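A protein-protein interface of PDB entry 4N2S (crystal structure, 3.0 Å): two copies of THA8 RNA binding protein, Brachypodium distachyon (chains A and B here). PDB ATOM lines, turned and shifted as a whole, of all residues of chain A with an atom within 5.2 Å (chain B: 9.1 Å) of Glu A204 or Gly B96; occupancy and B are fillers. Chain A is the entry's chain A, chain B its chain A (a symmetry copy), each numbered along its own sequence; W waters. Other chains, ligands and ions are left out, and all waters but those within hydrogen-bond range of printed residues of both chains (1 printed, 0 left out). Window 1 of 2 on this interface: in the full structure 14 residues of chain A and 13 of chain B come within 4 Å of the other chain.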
ATOM      1  N   VAL A 202      22.568  -9.300 -10.234  1.00  0.00           N
ATOM      2  CA  VAL A 202      22.502  -8.107 -11.058  1.00  0.00           C
ATOM      3  C   VAL A 202      23.885  -7.472 -11.220  1.00  0.00           C
ATOM      4  O   VAL A 202      24.887  -8.080 -10.824  1.00  0.00           O
ATOM      5  CB  VAL A 202      21.625  -7.066 -10.372  1.00  0.00           C
ATOM      6  CG1 VAL A 202      20.188  -7.530 -10.332  1.00  0.00           C
ATOM      7  CG2 VAL A 202      22.166  -6.802  -8.975  1.00  0.00           C
ATOM      8  N   ASP A 203      23.947  -6.267 -11.793  1.00  0.00           N
ATOM      9  CA  ASP A 203      25.222  -5.578 -12.019  1.00  0.00           C
ATOM     10  C   ASP A 203      25.347  -4.199 -11.424  1.00  0.00           C
ATOM     11  O   ASP A 203      24.456  -3.736 -10.694  1.00  0.00           O
ATOM     12  CB  ASP A 203      25.403  -5.403 -13.523  1.00  0.00           C
ATOM     13  CG  ASP A 203      24.229  -4.699 -14.191  1.00  0.00           C
ATOM     14  OD1 ASP A 203      23.323  -4.201 -13.479  1.00  0.00           O
ATOM     15  OD2 ASP A 203      24.223  -4.645 -15.446  1.00  0.00           O
ATOM     16  N   GLU A 204      26.479  -3.556 -11.723  1.00  0.00           N
ATOM     17  CA  GLU A 204      26.749  -2.214 -11.216  1.00  0.00           C
ATOM     18  C   GLU A 204      25.639  -1.207 -11.541  1.00  0.00           C
ATOM     19  O   GLU A 204      25.259  -0.384 -10.722  1.00  0.00           O
ATOM     20  CB  GLU A 204      28.097  -1.730 -11.734  1.00  0.00           C
ATOM     21  CG  GLU A 204      29.290  -2.563 -11.268  1.00  0.00           C
ATOM     22  CD  GLU A 204      30.579  -2.191 -12.005  1.00  0.00           C
ATOM     23  OE1 GLU A 204      30.613  -2.359 -13.232  1.00  0.00           O
ATOM     24  OE2 GLU A 204      31.556  -1.731 -11.384  1.00  0.00           O
ATOM     25  N   TYR A 205      25.118  -1.298 -12.751  1.00  0.00           N
ATOM     26  CA  TYR A 205      24.055  -0.420 -13.211  1.00  0.00           C
ATOM     27  C   TYR A 205      22.837  -0.580 -12.311  1.00  0.00           C
ATOM     28  O   TYR A 205      22.217   0.399 -11.925  1.00  0.00           O
ATOM     29  CB  TYR A 205      23.720  -0.802 -14.634  1.00  0.00           C
ATOM     30  CG  TYR A 205      22.829   0.130 -15.404  1.00  0.00           C
ATOM     31  CD1 TYR A 205      23.219   0.608 -16.644  1.00  0.00           C
ATOM     32  CD2 TYR A 205      21.563   0.461 -14.946  1.00  0.00           C
ATOM     33  CE1 TYR A 205      22.382   1.418 -17.395  1.00  0.00           C
ATOM     34  CE2 TYR A 205      20.733   1.286 -15.666  1.00  0.00           C
ATOM     35  CZ  TYR A 205      21.140   1.759 -16.878  1.00  0.00           C
ATOM     36  OH  TYR A 205      20.284   2.572 -17.562  1.00  0.00           O
ATOM     37  N   MET A 206      22.484  -1.809 -11.966  1.00  0.00           N
ATOM     38  CA  MET A 206      21.335  -2.015 -11.091  1.00  0.00           C
ATOM     39  C   MET A 206      21.528  -1.348  -9.720  1.00  0.00           C
ATOM     40  O   MET A 206      20.654  -0.615  -9.233  1.00  0.00           O
ATOM     41  CB  MET A 206      21.049  -3.499 -10.903  1.00  0.00           C
ATOM     42  CG  MET A 206      19.998  -3.799  -9.822  1.00  0.00           C
ATOM     43  SD  MET A 206      18.332  -3.161 -10.085  1.00  0.00           S
ATOM     44  CE  MET A 206      17.500  -4.595 -10.782  1.00  0.00           C
ATOM     45  N   TYR A 207      22.679  -1.612  -9.108  1.00  0.00           N
ATOM     46  CA  TYR A 207      22.968  -1.076  -7.786  1.00  0.00           C
ATOM     47  C   TYR A 207      22.929   0.431  -7.818  1.00  0.00           C
ATOM     48  O   TYR A 207      22.293   1.066  -6.977  1.00  0.00           O
ATOM     49  CB  TYR A 207      24.336  -1.564  -7.287  1.00  0.00           C
ATOM     50  CG  TYR A 207      24.379  -3.054  -7.022  1.00  0.00           C
ATOM     51  CD1 TYR A 207      23.520  -3.650  -6.096  1.00  0.00           C
ATOM     52  CD2 TYR A 207      25.275  -3.874  -7.713  1.00  0.00           C
ATOM     53  CE1 TYR A 207      23.537  -5.028  -5.875  1.00  0.00           C
ATOM     54  CE2 TYR A 207      25.323  -5.257  -7.500  1.00  0.00           C
ATOM     55  CZ  TYR A 207      24.460  -5.831  -6.576  1.00  0.00           C
ATOM     56  OH  TYR A 207      24.515  -7.202  -6.399  1.00  0.00           O
ATOM     57  N   ARG A 208      23.609   0.992  -8.815  1.00  0.00           N
ATOM     58  CA  ARG A 208      23.702   2.434  -8.962  1.00  0.00           C
ATOM     59  C   ARG A 208      22.302   3.041  -9.002  1.00  0.00           C
ATOM     60  O   ARG A 208      22.043   4.072  -8.381  1.00  0.00           O
ATOM     61  CB  ARG A 208      24.506   2.783 -10.210  1.00  0.00           C
ATOM     62  CG  ARG A 208      25.577   3.850  -9.993  1.00  0.00           C
ATOM     63  CD  ARG A 208      25.727   4.788 -11.202  1.00  0.00           C
ATOM     64  NE  ARG A 208      24.527   5.597 -11.510  1.00  0.00           N
ATOM     65  CZ  ARG A 208      23.494   5.216 -12.285  1.00  0.00           C
ATOM     66  NH1 ARG A 208      23.457   4.017 -12.875  1.00  0.00           N
ATOM     67  NH2 ARG A 208      22.483   6.057 -12.483  1.00  0.00           N
ATOM     68  N   VAL A 209      21.394   2.367  -9.701  1.00  0.00           N
ATOM     69  CA  VAL A 209      20.002   2.826  -9.812  1.00  0.00           C
ATOM     70  C   VAL A 209      19.319   2.831  -8.443  1.00  0.00           C
ATOM     71  O   VAL A 209      18.706   3.824  -8.062  1.00  0.00           O
ATOM     72  CB  VAL A 209      19.197   1.967 -10.820  1.00  0.00           C
ATOM     73  CG1 VAL A 209      17.710   2.270 -10.743  1.00  0.00           C
ATOM     74  CG2 VAL A 209      19.688   2.219 -12.224  1.00  0.00           C
ATOM     75  N   LEU A 230      26.667  -3.696  -3.188  1.00  0.00           N
ATOM     76  CA  LEU A 230      27.555  -3.336  -4.287  1.00  0.00           C
ATOM     77  C   LEU A 230      28.995  -3.537  -3.830  1.00  0.00           C
ATOM     78  O   LEU A 230      29.816  -4.071  -4.577  1.00  0.00           O
ATOM     79  CB  LEU A 230      27.353  -1.875  -4.699  1.00  0.00           C
ATOM     80  CG  LEU A 230      28.311  -1.348  -5.768  1.00  0.00           C
ATOM     81  CD1 LEU A 230      28.155  -2.094  -7.094  1.00  0.00           C
ATOM     82  CD2 LEU A 230      27.967   0.129  -5.958  1.00  0.00           C
ATOM     83  N   TRP A 233      29.713  -6.796  -4.100  1.00  0.00           N
ATOM     84  CA  TRP A 233      29.752  -7.149  -5.518  1.00  0.00           C
ATOM     85  C   TRP A 233      31.127  -6.804  -6.080  1.00  0.00           C
ATOM     86  O   TRP A 233      31.783  -7.631  -6.726  1.00  0.00           O
ATOM     87  CB  TRP A 233      28.654  -6.373  -6.279  1.00  0.00           C
ATOM     88  CG  TRP A 233      28.494  -6.818  -7.706  1.00  0.00           C
ATOM     89  CD1 TRP A 233      27.598  -7.742  -8.202  1.00  0.00           C
ATOM     90  CD2 TRP A 233      29.295  -6.391  -8.848  1.00  0.00           C
ATOM     91  NE1 TRP A 233      27.791  -7.929  -9.540  1.00  0.00           N
ATOM     92  CE2 TRP A 233      28.799  -7.139  -9.993  1.00  0.00           C
ATOM     93  CE3 TRP A 233      30.344  -5.504  -9.023  1.00  0.00           C
ATOM     94  CZ2 TRP A 233      29.338  -6.983 -11.258  1.00  0.00           C
ATOM     95  CZ3 TRP A 233      30.883  -5.354 -10.300  1.00  0.00           C
ATOM     96  CH2 TRP A 233      30.388  -6.085 -11.393  1.00  0.00           C
ATOM     97  N   GLU A 234      31.554  -5.586  -5.816  1.00  0.00           N
ATOM     98  CA  GLU A 234      32.801  -5.089  -6.326  1.00  0.00           C
ATOM     99  C   GLU A 234      33.943  -5.834  -5.714  1.00  0.00           C
ATOM    100  O   GLU A 234      35.046  -5.764  -6.186  1.00  0.00           O
ATOM    101  CB  GLU A 234      32.945  -3.615  -5.998  1.00  0.00           C
ATOM    102  CG  GLU A 234      32.033  -2.707  -6.762  1.00  0.00           C
ATOM    103  CD  GLU A 234      32.454  -2.534  -8.182  1.00  0.00           C
ATOM    104  OE1 GLU A 234      33.572  -2.923  -8.516  1.00  0.00           O
ATOM    105  OE2 GLU A 234      31.672  -2.004  -8.975  1.00  0.00           O
ATOM    106  N   LYS B  57      28.518  -4.965 -23.200  1.00  0.00           N
ATOM    107  CA  LYS B  57      27.493  -5.282 -22.202  1.00  0.00           C
ATOM    108  C   LYS B  57      26.772  -6.591 -22.529  1.00  0.00           C
ATOM    109  O   LYS B  57      26.629  -7.457 -21.663  1.00  0.00           O
ATOM    110  CB  LYS B  57      26.477  -4.130 -22.062  1.00  0.00           C
ATOM    111  CG  LYS B  57      27.103  -2.780 -21.744  1.00  0.00           C
ATOM    112  CD  LYS B  57      26.089  -1.813 -21.153  1.00  0.00           C
ATOM    113  CE  LYS B  57      24.993  -1.445 -22.139  1.00  0.00           C
ATOM    114  NZ  LYS B  57      23.962  -0.534 -21.590  1.00  0.00           N
ATOM    115  N   THR B  60      29.244  -9.478 -21.688  1.00  0.00           N
ATOM    116  CA  THR B  60      29.419  -9.690 -20.255  1.00  0.00           C
ATOM    117  C   THR B  60      28.092 -10.048 -19.569  1.00  0.00           C
ATOM    118  O   THR B  60      28.083 -10.549 -18.431  1.00  0.00           O
ATOM    119  CB  THR B  60      30.023  -8.436 -19.595  1.00  0.00           C
ATOM    120  OG1 THR B  60      29.202  -7.287 -19.897  1.00  0.00           O
ATOM    121  CG2 THR B  60      31.429  -8.199 -20.115  1.00  0.00           C
ATOM    122  N   ARG B  64      29.919 -12.363 -16.056  1.00  0.00           N
ATOM    123  CA  ARG B  64      30.319 -11.125 -15.427  1.00  0.00           C
ATOM    124  C   ARG B  64      31.657 -11.220 -14.700  1.00  0.00           C
ATOM    125  O   ARG B  64      32.195 -10.211 -14.252  1.00  0.00           O
ATOM    126  CB  ARG B  64      29.216 -10.654 -14.475  1.00  0.00           C
ATOM    127  CG  ARG B  64      27.853 -10.431 -15.139  1.00  0.00           C
ATOM    128  CD  ARG B  64      26.866  -9.876 -14.142  1.00  0.00           C
ATOM    129  NE  ARG B  64      25.494 -10.079 -14.588  1.00  0.00           N
ATOM    130  CZ  ARG B  64      24.876  -9.340 -15.510  1.00  0.00           C
ATOM    131  NH1 ARG B  64      25.506  -8.337 -16.097  1.00  0.00           N
ATOM    132  NH2 ARG B  64      23.617  -9.596 -15.836  1.00  0.00           N
ATOM    133  N   ALA B  69      35.415 -10.457 -18.455  1.00  0.00           N
ATOM    134  CA  ALA B  69      35.215  -9.033 -18.667  1.00  0.00           C
ATOM    135  C   ALA B  69      36.297  -8.473 -19.591  1.00  0.00           C
ATOM    136  O   ALA B  69      36.010  -7.979 -20.689  1.00  0.00           O
ATOM    137  CB  ALA B  69      35.222  -8.299 -17.343  1.00  0.00           C
ATOM    138  N   MET B  89      34.782   4.482 -22.809  1.00  0.00           N
ATOM    139  CA  MET B  89      35.261   4.314 -21.454  1.00  0.00           C
ATOM    140  C   MET B  89      34.439   5.180 -20.490  1.00  0.00           C
ATOM    141  O   MET B  89      33.940   4.697 -19.468  1.00  0.00           O
ATOM    142  CB  MET B  89      36.725   4.709 -21.390  1.00  0.00           C
ATOM    143  CG  MET B  89      37.416   4.258 -20.137  1.00  0.00           C
ATOM    144  SD  MET B  89      39.050   4.977 -20.064  1.00  0.00           S
ATOM    145  CE  MET B  89      39.844   4.311 -21.540  1.00  0.00           C
ATOM    146  N   ALA B  90      34.309   6.461 -20.831  1.00  0.00           N
ATOM    147  CA  ALA B  90      33.570   7.437 -20.036  1.00  0.00           C
ATOM    148  C   ALA B  90      32.074   7.150 -20.064  1.00  0.00           C
ATOM    149  O   ALA B  90      31.348   7.508 -19.136  1.00  0.00           O
ATOM    150  CB  ALA B  90      33.851   8.833 -20.545  1.00  0.00           C
ATOM    151  N   GLU B  91      31.610   6.493 -21.125  1.00  0.00           N
ATOM    152  CA  GLU B  91      30.194   6.156 -21.239  1.00  0.00           C
ATOM    153  C   GLU B  91      29.820   5.068 -20.258  1.00  0.00           C
ATOM    154  O   GLU B  91      28.735   5.075 -19.687  1.00  0.00           O
ATOM    155  CB  GLU B  91      29.878   5.707 -22.654  1.00  0.00           C
ATOM    156  CG  GLU B  91      28.401   5.331 -22.857  1.00  0.00           C
ATOM    157  CD  GLU B  91      27.402   6.318 -22.253  1.00  0.00           C
ATOM    158  OE1 GLU B  91      27.754   7.504 -22.003  1.00  0.00           O
ATOM    159  OE2 GLU B  91      26.245   5.901 -22.035  1.00  0.00           O
ATOM    160  N   LEU B  92      30.746   4.127 -20.084  1.00  0.00           N
ATOM    161  CA  LEU B  92      30.596   3.034 -19.128  1.00  0.00           C
ATOM    162  C   LEU B  92      30.625   3.623 -17.741  1.00  0.00           C
ATOM    163  O   LEU B  92      29.815   3.245 -16.907  1.00  0.00           O
ATOM    164  CB  LEU B  92      31.722   2.007 -19.288  1.00  0.00           C
ATOM    165  CG  LEU B  92      31.731   1.239 -20.607  1.00  0.00           C
ATOM    166  CD1 LEU B  92      32.991   0.435 -20.725  1.00  0.00           C
ATOM    167  CD2 LEU B  92      30.523   0.330 -20.678  1.00  0.00           C
ATOM    168  N   GLN B  93      31.545   4.556 -17.495  1.00  0.00           N
ATOM    169  CA  GLN B  93      31.650   5.180 -16.173  1.00  0.00           C
ATOM    170  C   GLN B  93      30.308   5.821 -15.844  1.00  0.00           C
ATOM    171  O   GLN B  93      29.767   5.619 -14.767  1.00  0.00           O
ATOM    172  CB  GLN B  93      32.716   6.267 -16.134  1.00  0.00           C
ATOM    173  CG  GLN B  93      34.104   5.837 -16.491  1.00  0.00           C
ATOM    174  CD  GLN B  93      35.080   7.004 -16.386  1.00  0.00           C
ATOM    175  OE1 GLN B  93      34.909   8.046 -17.022  1.00  0.00           O
ATOM    176  NE2 GLN B  93      36.122   6.832 -15.578  1.00  0.00           N
ATOM    177  N   ARG B  94      29.795   6.592 -16.803  1.00  0.00           N
ATOM    178  CA  ARG B  94      28.542   7.326 -16.678  1.00  0.00           C
ATOM    179  C   ARG B  94      27.376   6.415 -16.297  1.00  0.00           C
ATOM    180  O   ARG B  94      26.516   6.787 -15.502  1.00  0.00           O
ATOM    181  CB  ARG B  94      28.240   8.035 -17.999  1.00  0.00           C
ATOM    182  CG  ARG B  94      26.952   8.847 -18.036  1.00  0.00           C
ATOM    183  CD  ARG B  94      26.530   9.164 -19.490  1.00  0.00           C
ATOM    184  NE  ARG B  94      25.672   8.126 -20.081  1.00  0.00           N
ATOM    185  CZ  ARG B  94      24.367   7.982 -19.827  1.00  0.00           C
ATOM    186  NH1 ARG B  94      23.746   8.829 -19.001  1.00  0.00           N
ATOM    187  NH2 ARG B  94      23.682   6.986 -20.386  1.00  0.00           N
ATOM    188  N   GLN B  95      27.365   5.215 -16.870  1.00  0.00           N
ATOM    189  CA  GLN B  95      26.313   4.234 -16.621  1.00  0.00           C
ATOM    190  C   GLN B  95      26.456   3.496 -15.283  1.00  0.00           C
ATOM    191  O   GLN B  95      25.543   2.765 -14.866  1.00  0.00           O
ATOM    192  CB  GLN B  95      26.275   3.221 -17.766  1.00  0.00           C
ATOM    193  CG  GLN B  95      25.798   3.831 -19.063  1.00  0.00           C
ATOM    194  CD  GLN B  95      25.534   2.791 -20.146  1.00  0.00           C
ATOM    195  OE1 GLN B  95      25.324   1.598 -19.882  1.00  0.00           O
ATOM    196  NE2 GLN B  95      25.531   3.250 -21.391  1.00  0.00           N
ATOM    197  N   GLY B  96      27.603   3.668 -14.629  1.00  0.00           N
ATOM    198  CA  GLY B  96      27.860   3.002 -13.375  1.00  0.00           C
ATOM    199  C   GLY B  96      28.642   1.713 -13.504  1.00  0.00           C
ATOM    200  O   GLY B  96      28.976   1.086 -12.494  1.00  0.00           O
ATOM    201  N   HIS B  97      28.913   1.294 -14.738  1.00  0.00           N
ATOM    202  CA  HIS B  97      29.717   0.092 -14.997  1.00  0.00           C
ATOM    203  C   HIS B  97      31.193   0.400 -14.810  1.00  0.00           C
ATOM    204  O   HIS B  97      31.976   0.426 -15.756  1.00  0.00           O
ATOM    205  CB  HIS B  97      29.448  -0.463 -16.386  1.00  0.00           C
ATOM    206  CG  HIS B  97      28.070  -1.023 -16.572  1.00  0.00           C
ATOM    207  ND1 HIS B  97      27.679  -2.191 -16.027  1.00  0.00           N
ATOM    208  CD2 HIS B  97      26.983  -0.539 -17.293  1.00  0.00           C
ATOM    209  CE1 HIS B  97      26.399  -2.444 -16.387  1.00  0.00           C
ATOM    210  NE2 HIS B  97      25.978  -1.433 -17.157  1.00  0.00           N
ATOM    211  N   TRP B  98      31.574   0.647 -13.561  1.00  0.00           N
ATOM    212  CA  TRP B  98      32.941   1.013 -13.204  1.00  0.00           C
ATOM    213  C   TRP B  98      33.931  -0.101 -13.503  1.00  0.00           C
ATOM    214  O   TRP B  98      35.030   0.141 -14.035  1.00  0.00           O
ATOM    215  CB  TRP B  98      32.967   1.428 -11.739  1.00  0.00           C
ATOM    216  CG  TRP B  98      34.089   2.315 -11.382  1.00  0.00           C
ATOM    217  CD1 TRP B  98      34.340   3.578 -11.866  1.00  0.00           C
ATOM    218  CD2 TRP B  98      35.162   2.022 -10.452  1.00  0.00           C
ATOM    219  NE1 TRP B  98      35.487   4.090 -11.306  1.00  0.00           N
ATOM    220  CE2 TRP B  98      36.022   3.188 -10.443  1.00  0.00           C
ATOM    221  CE3 TRP B  98      35.490   0.931  -9.656  1.00  0.00           C
ATOM    222  CZ2 TRP B  98      37.150   3.250  -9.654  1.00  0.00           C
ATOM    223  CZ3 TRP B  98      36.631   0.997  -8.862  1.00  0.00           C
ATOM    224  CH2 TRP B  98      37.439   2.132  -8.858  1.00  0.00           C
ATOM    225  N   SER B  99      33.576  -1.338 -13.167  1.00  0.00           N
ATOM    226  CA  SER B  99      34.504  -2.445 -13.401  1.00  0.00           C
ATOM    227  C   SER B  99      34.791  -2.547 -14.897  1.00  0.00           C
ATOM    228  O   SER B  99      35.919  -2.804 -15.307  1.00  0.00           O
ATOM    229  CB  SER B  99      33.930  -3.746 -12.869  1.00  0.00           C
ATOM    230  OG  SER B  99      32.755  -4.096 -13.576  1.00  0.00           O
ATOM    231  N   LEU B 100      33.764  -2.327 -15.705  1.00  0.00           N
ATOM    232  CA  LEU B 100      33.906  -2.411 -17.151  1.00  0.00           C
ATOM    233  C   LEU B 100      34.695  -1.226 -17.681  1.00  0.00           C
ATOM    234  O   LEU B 100      35.337  -1.331 -18.727  1.00  0.00           O
ATOM    235  CB  LEU B 100      32.541  -2.436 -17.842  1.00  0.00           C
ATOM    236  CG  LEU B 100      31.573  -3.529 -17.352  1.00  0.00           C
ATOM    237  CD1 LEU B 100      30.326  -3.549 -18.225  1.00  0.00           C
ATOM    238  CD2 LEU B 100      32.286  -4.880 -17.357  1.00  0.00           C
ATOM    239  N   ALA B 101      34.632  -0.098 -16.963  1.00  0.00           N
ATOM    240  CA  ALA B 101      35.378   1.094 -17.339  1.00  0.00           C
ATOM    241  C   ALA B 101      36.877   0.829 -17.111  1.00  0.00           C
ATOM    242  O   ALA B 101      37.730   1.206 -17.919  1.00  0.00           O
ATOM    243  CB  ALA B 101      34.892   2.281 -16.526  1.00  0.00           C
ATOM    244  N   LEU B 102      37.185   0.155 -15.997  1.00  0.00           N
ATOM    245  CA  LEU B 102      38.551  -0.240 -15.671  1.00  0.00           C
ATOM    246  C   LEU B 102      39.079  -1.198 -16.747  1.00  0.00           C
ATOM    247  O   LEU B 102      40.263  -1.168 -17.077  1.00  0.00           O
ATOM    248  CB  LEU B 102      38.577  -0.939 -14.326  1.00  0.00           C
ATOM    249  CG  LEU B 102      38.348  -0.033 -13.146  1.00  0.00           C
ATOM    250  CD1 LEU B 102      38.256  -0.858 -11.877  1.00  0.00           C
ATOM    251  CD2 LEU B 102      39.527   0.927 -13.084  1.00  0.00           C
ATOM    252  N   ALA B 103      38.206  -2.067 -17.269  1.00  0.00           N
ATOM    253  CA  ALA B 103      38.578  -2.975 -18.335  1.00  0.00           C
ATOM    254  C   ALA B 103      38.963  -2.175 -19.600  1.00  0.00           C
ATOM    255  O   ALA B 103      39.961  -2.469 -20.274  1.00  0.00           O
ATOM    256  CB  ALA B 103      37.431  -3.921 -18.630  1.00  0.00           C
ATOM    257  N   PHE B 124      37.863   8.257 -13.399  1.00  0.00           N
ATOM    258  CA  PHE B 124      37.712   7.017 -12.663  1.00  0.00           C
ATOM    259  C   PHE B 124      37.460   7.241 -11.170  1.00  0.00           C
ATOM    260  O   PHE B 124      36.565   6.616 -10.588  1.00  0.00           O
ATOM    261  CB  PHE B 124      38.950   6.143 -12.837  1.00  0.00           C
ATOM    262  CG  PHE B 124      38.887   5.259 -14.039  1.00  0.00           C
ATOM    263  CD1 PHE B 124      38.017   4.156 -14.055  1.00  0.00           C
ATOM    264  CD2 PHE B 124      39.654   5.536 -15.176  1.00  0.00           C
ATOM    265  CE1 PHE B 124      37.932   3.345 -15.187  1.00  0.00           C
ATOM    266  CE2 PHE B 124      39.577   4.727 -16.297  1.00  0.00           C
ATOM    267  CZ  PHE B 124      38.714   3.626 -16.301  1.00  0.00           C
ATOM    268  N   SER B 127      33.936   8.674 -10.723  1.00  0.00           N
ATOM    269  CA  SER B 127      32.873   7.744 -11.013  1.00  0.00           C
ATOM    270  C   SER B 127      32.939   6.472 -10.202  1.00  0.00           C
ATOM    271  O   SER B 127      32.263   5.496 -10.549  1.00  0.00           O
ATOM    272  CB  SER B 127      32.875   7.384 -12.485  1.00  0.00           C
ATOM    273  OG  SER B 127      34.081   6.777 -12.874  1.00  0.00           O
ATOM    274  N   SER B 128      33.745   6.458  -9.142  1.00  0.00           N
ATOM    275  CA  SER B 128      33.865   5.269  -8.312  1.00  0.00           C
ATOM    276  C   SER B 128      32.711   5.230  -7.276  1.00  0.00           C
ATOM    277  O   SER B 128      32.281   6.290  -6.794  1.00  0.00           O
ATOM    278  CB  SER B 128      35.235   5.223  -7.632  1.00  0.00           C
ATOM    279  OG  SER B 128      35.310   6.170  -6.604  1.00  0.00           O
ATOM    280  N   PRO B 129      32.204   4.004  -6.945  1.00  0.00           N
ATOM    281  CA  PRO B 129      31.131   3.791  -5.962  1.00  0.00           C
ATOM    282  C   PRO B 129      31.551   4.213  -4.563  1.00  0.00           C
ATOM    283  O   PRO B 129      32.560   3.733  -4.032  1.00  0.00           O
ATOM    284  CB  PRO B 129      30.916   2.272  -6.029  1.00  0.00           C
ATOM    285  CG  PRO B 129      31.321   1.913  -7.418  1.00  0.00           C
ATOM    286  CD  PRO B 129      32.565   2.729  -7.597  1.00  0.00           C
ATOM    287  N   ASP B 132      32.614   2.115  -0.629  1.00  0.00           N
ATOM    288  CA  ASP B 132      33.046   0.822  -1.176  1.00  0.00           C
ATOM    289  C   ASP B 132      34.502   0.562  -0.862  1.00  0.00           C
ATOM    290  O   ASP B 132      35.386   1.088  -1.545  1.00  0.00           O
ATOM    291  CB  ASP B 132      32.871   0.790  -2.690  1.00  0.00           C
ATOM    292  CG  ASP B 132      31.665   0.011  -3.121  1.00  0.00           C
ATOM    293  OD1 ASP B 132      30.503   0.428  -2.794  1.00  0.00           O
ATOM    294  OD2 ASP B 132      31.927  -1.008  -3.811  1.00  0.00           O
ATOM    295  N   ALA B 135      36.387  -0.689  -3.862  1.00  0.00           N
ATOM    296  CA  ALA B 135      36.611   0.397  -4.803  1.00  0.00           C
ATOM    297  C   ALA B 135      37.653   1.370  -4.270  1.00  0.00           C
ATOM    298  O   ALA B 135      38.506   1.839  -5.027  1.00  0.00           O
ATOM    299  CB  ALA B 135      35.307   1.127  -5.082  1.00  0.00           C
HETATM  300  O   HOH W   1      25.158  -6.179 -18.025  1.00  0.00           O
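The guanidinium group of Arg A208 lies within hydrogen-bond range of the backbone carbonyl oxygen of Gln B95, 3.1 Å away. The guanidinium group (NH1) of Arg B64 lies within salt-bridge range of the side-chain carboxylate (OD2) of Asp A203 (3.96 Å). OE2 of Glu A204 sits at hydrogen-bond distance from N of Ser B99 (2.7 Å). The side-chain carboxylate (OE1) of Glu A204 lies within hydrogen-bond range of the backbone NH (N) of Trp B98, 3.2 Å away.
OD1 of Asp A203 sits at hydrogen-bond distance from N of Met A206 (3.0 Å). NZ of Lys B57 is in hydrogen-bond range of OE1 of Gln B95, 3.1 Å away. The side-chain amide nitrogen (NE2) of Gln B95 sits at hydrogen-bond distance from the side-chain carboxylate (OE2) of Glu B91. O of Leu B92 lies within hydrogen-bond range of N of His B97 (3.1 Å). The backbone carbonyl oxygen of Phe B124 lies within hydrogen-bond range of the indole nitrogen of Trp B98 (2.8 Å). The side-chain carboxylate of Glu A234 sits close to the side-chain carboxylate of Glu A204 (2.4 Å).
His B97 touches Asp A203. Glu A204 touches Gly B96. His B97 touches Glu A204. Gln B95 touches Tyr A205 (O to CD1, 3.6 Å). NE2 of His B97 touches CB of Tyr A205, 3.4 Å away. CA of Gly B96 touches CD of Arg A208, 3.5 Å away. Pro B129 touches Leu A230 (CB to CD2, 3.6 Å). Leu A230 touches Asp B132. Trp A233 touches Ser B99 (CH2 to OG, 3.8 Å). Glu A234 touches Asp B132.
Of chain A, only Glu A204 and Arg A208 come within 4 Å of Gly B96. Printed residues of chain B within 4 Å of Asp A203: Arg B64 (3.9 Å) and His B97 (3.2 Å). Of the printed residues of chain A, His B97 touches Asp A203, Glu A204 and Tyr A205. Printed residues of chain A within 4 Å of Gln B95: Tyr A205 (3.6 Å) and Arg A208 (3.1 Å). Of the printed residues of chain A, Pro B129 touches Leu A230. Printed residues of chain B within 4 Å of Leu A230: Pro B129 (3.6 Å) and Asp B132 (3.8 Å). Of the printed residues of chain B, Tyr A205 touches Gln B95 (3.6 Å) and His B97 (3.4 Å). Val A209 touches none of the printed residues of chain B. Val A202 touches none of the printed residues of chain B. The nearest printed residue of chain A that does not touch Gln B95 is Glu A204 (5.2 Å).
Of the 11 printed residues of chain A, 7 touch a printed residue of chain B. Hydrophobic or aromatic side chains of chain A that line the printed part of chain B: Tyr A205, Leu A230 and Trp A233. Of the 25 printed residues of chain B, 8 touch a printed residue of chain A. Among the printed residues, Asp or Glu carboxylates within 4 Å of a Lys or Arg side-chain nitrogen of the other chain: Asp A203 with Arg B64.
No position is printed for both chains. Of the 14 pairs that touch across the chains among the printed residues, none has its exchanged pair printed and touching as well.
Water W1 lies within hydrogen-bond range of the guanidinium group of Arg B64 (2.9 Å) and the side-chain carboxylate of Asp A203 (3.1 Å).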
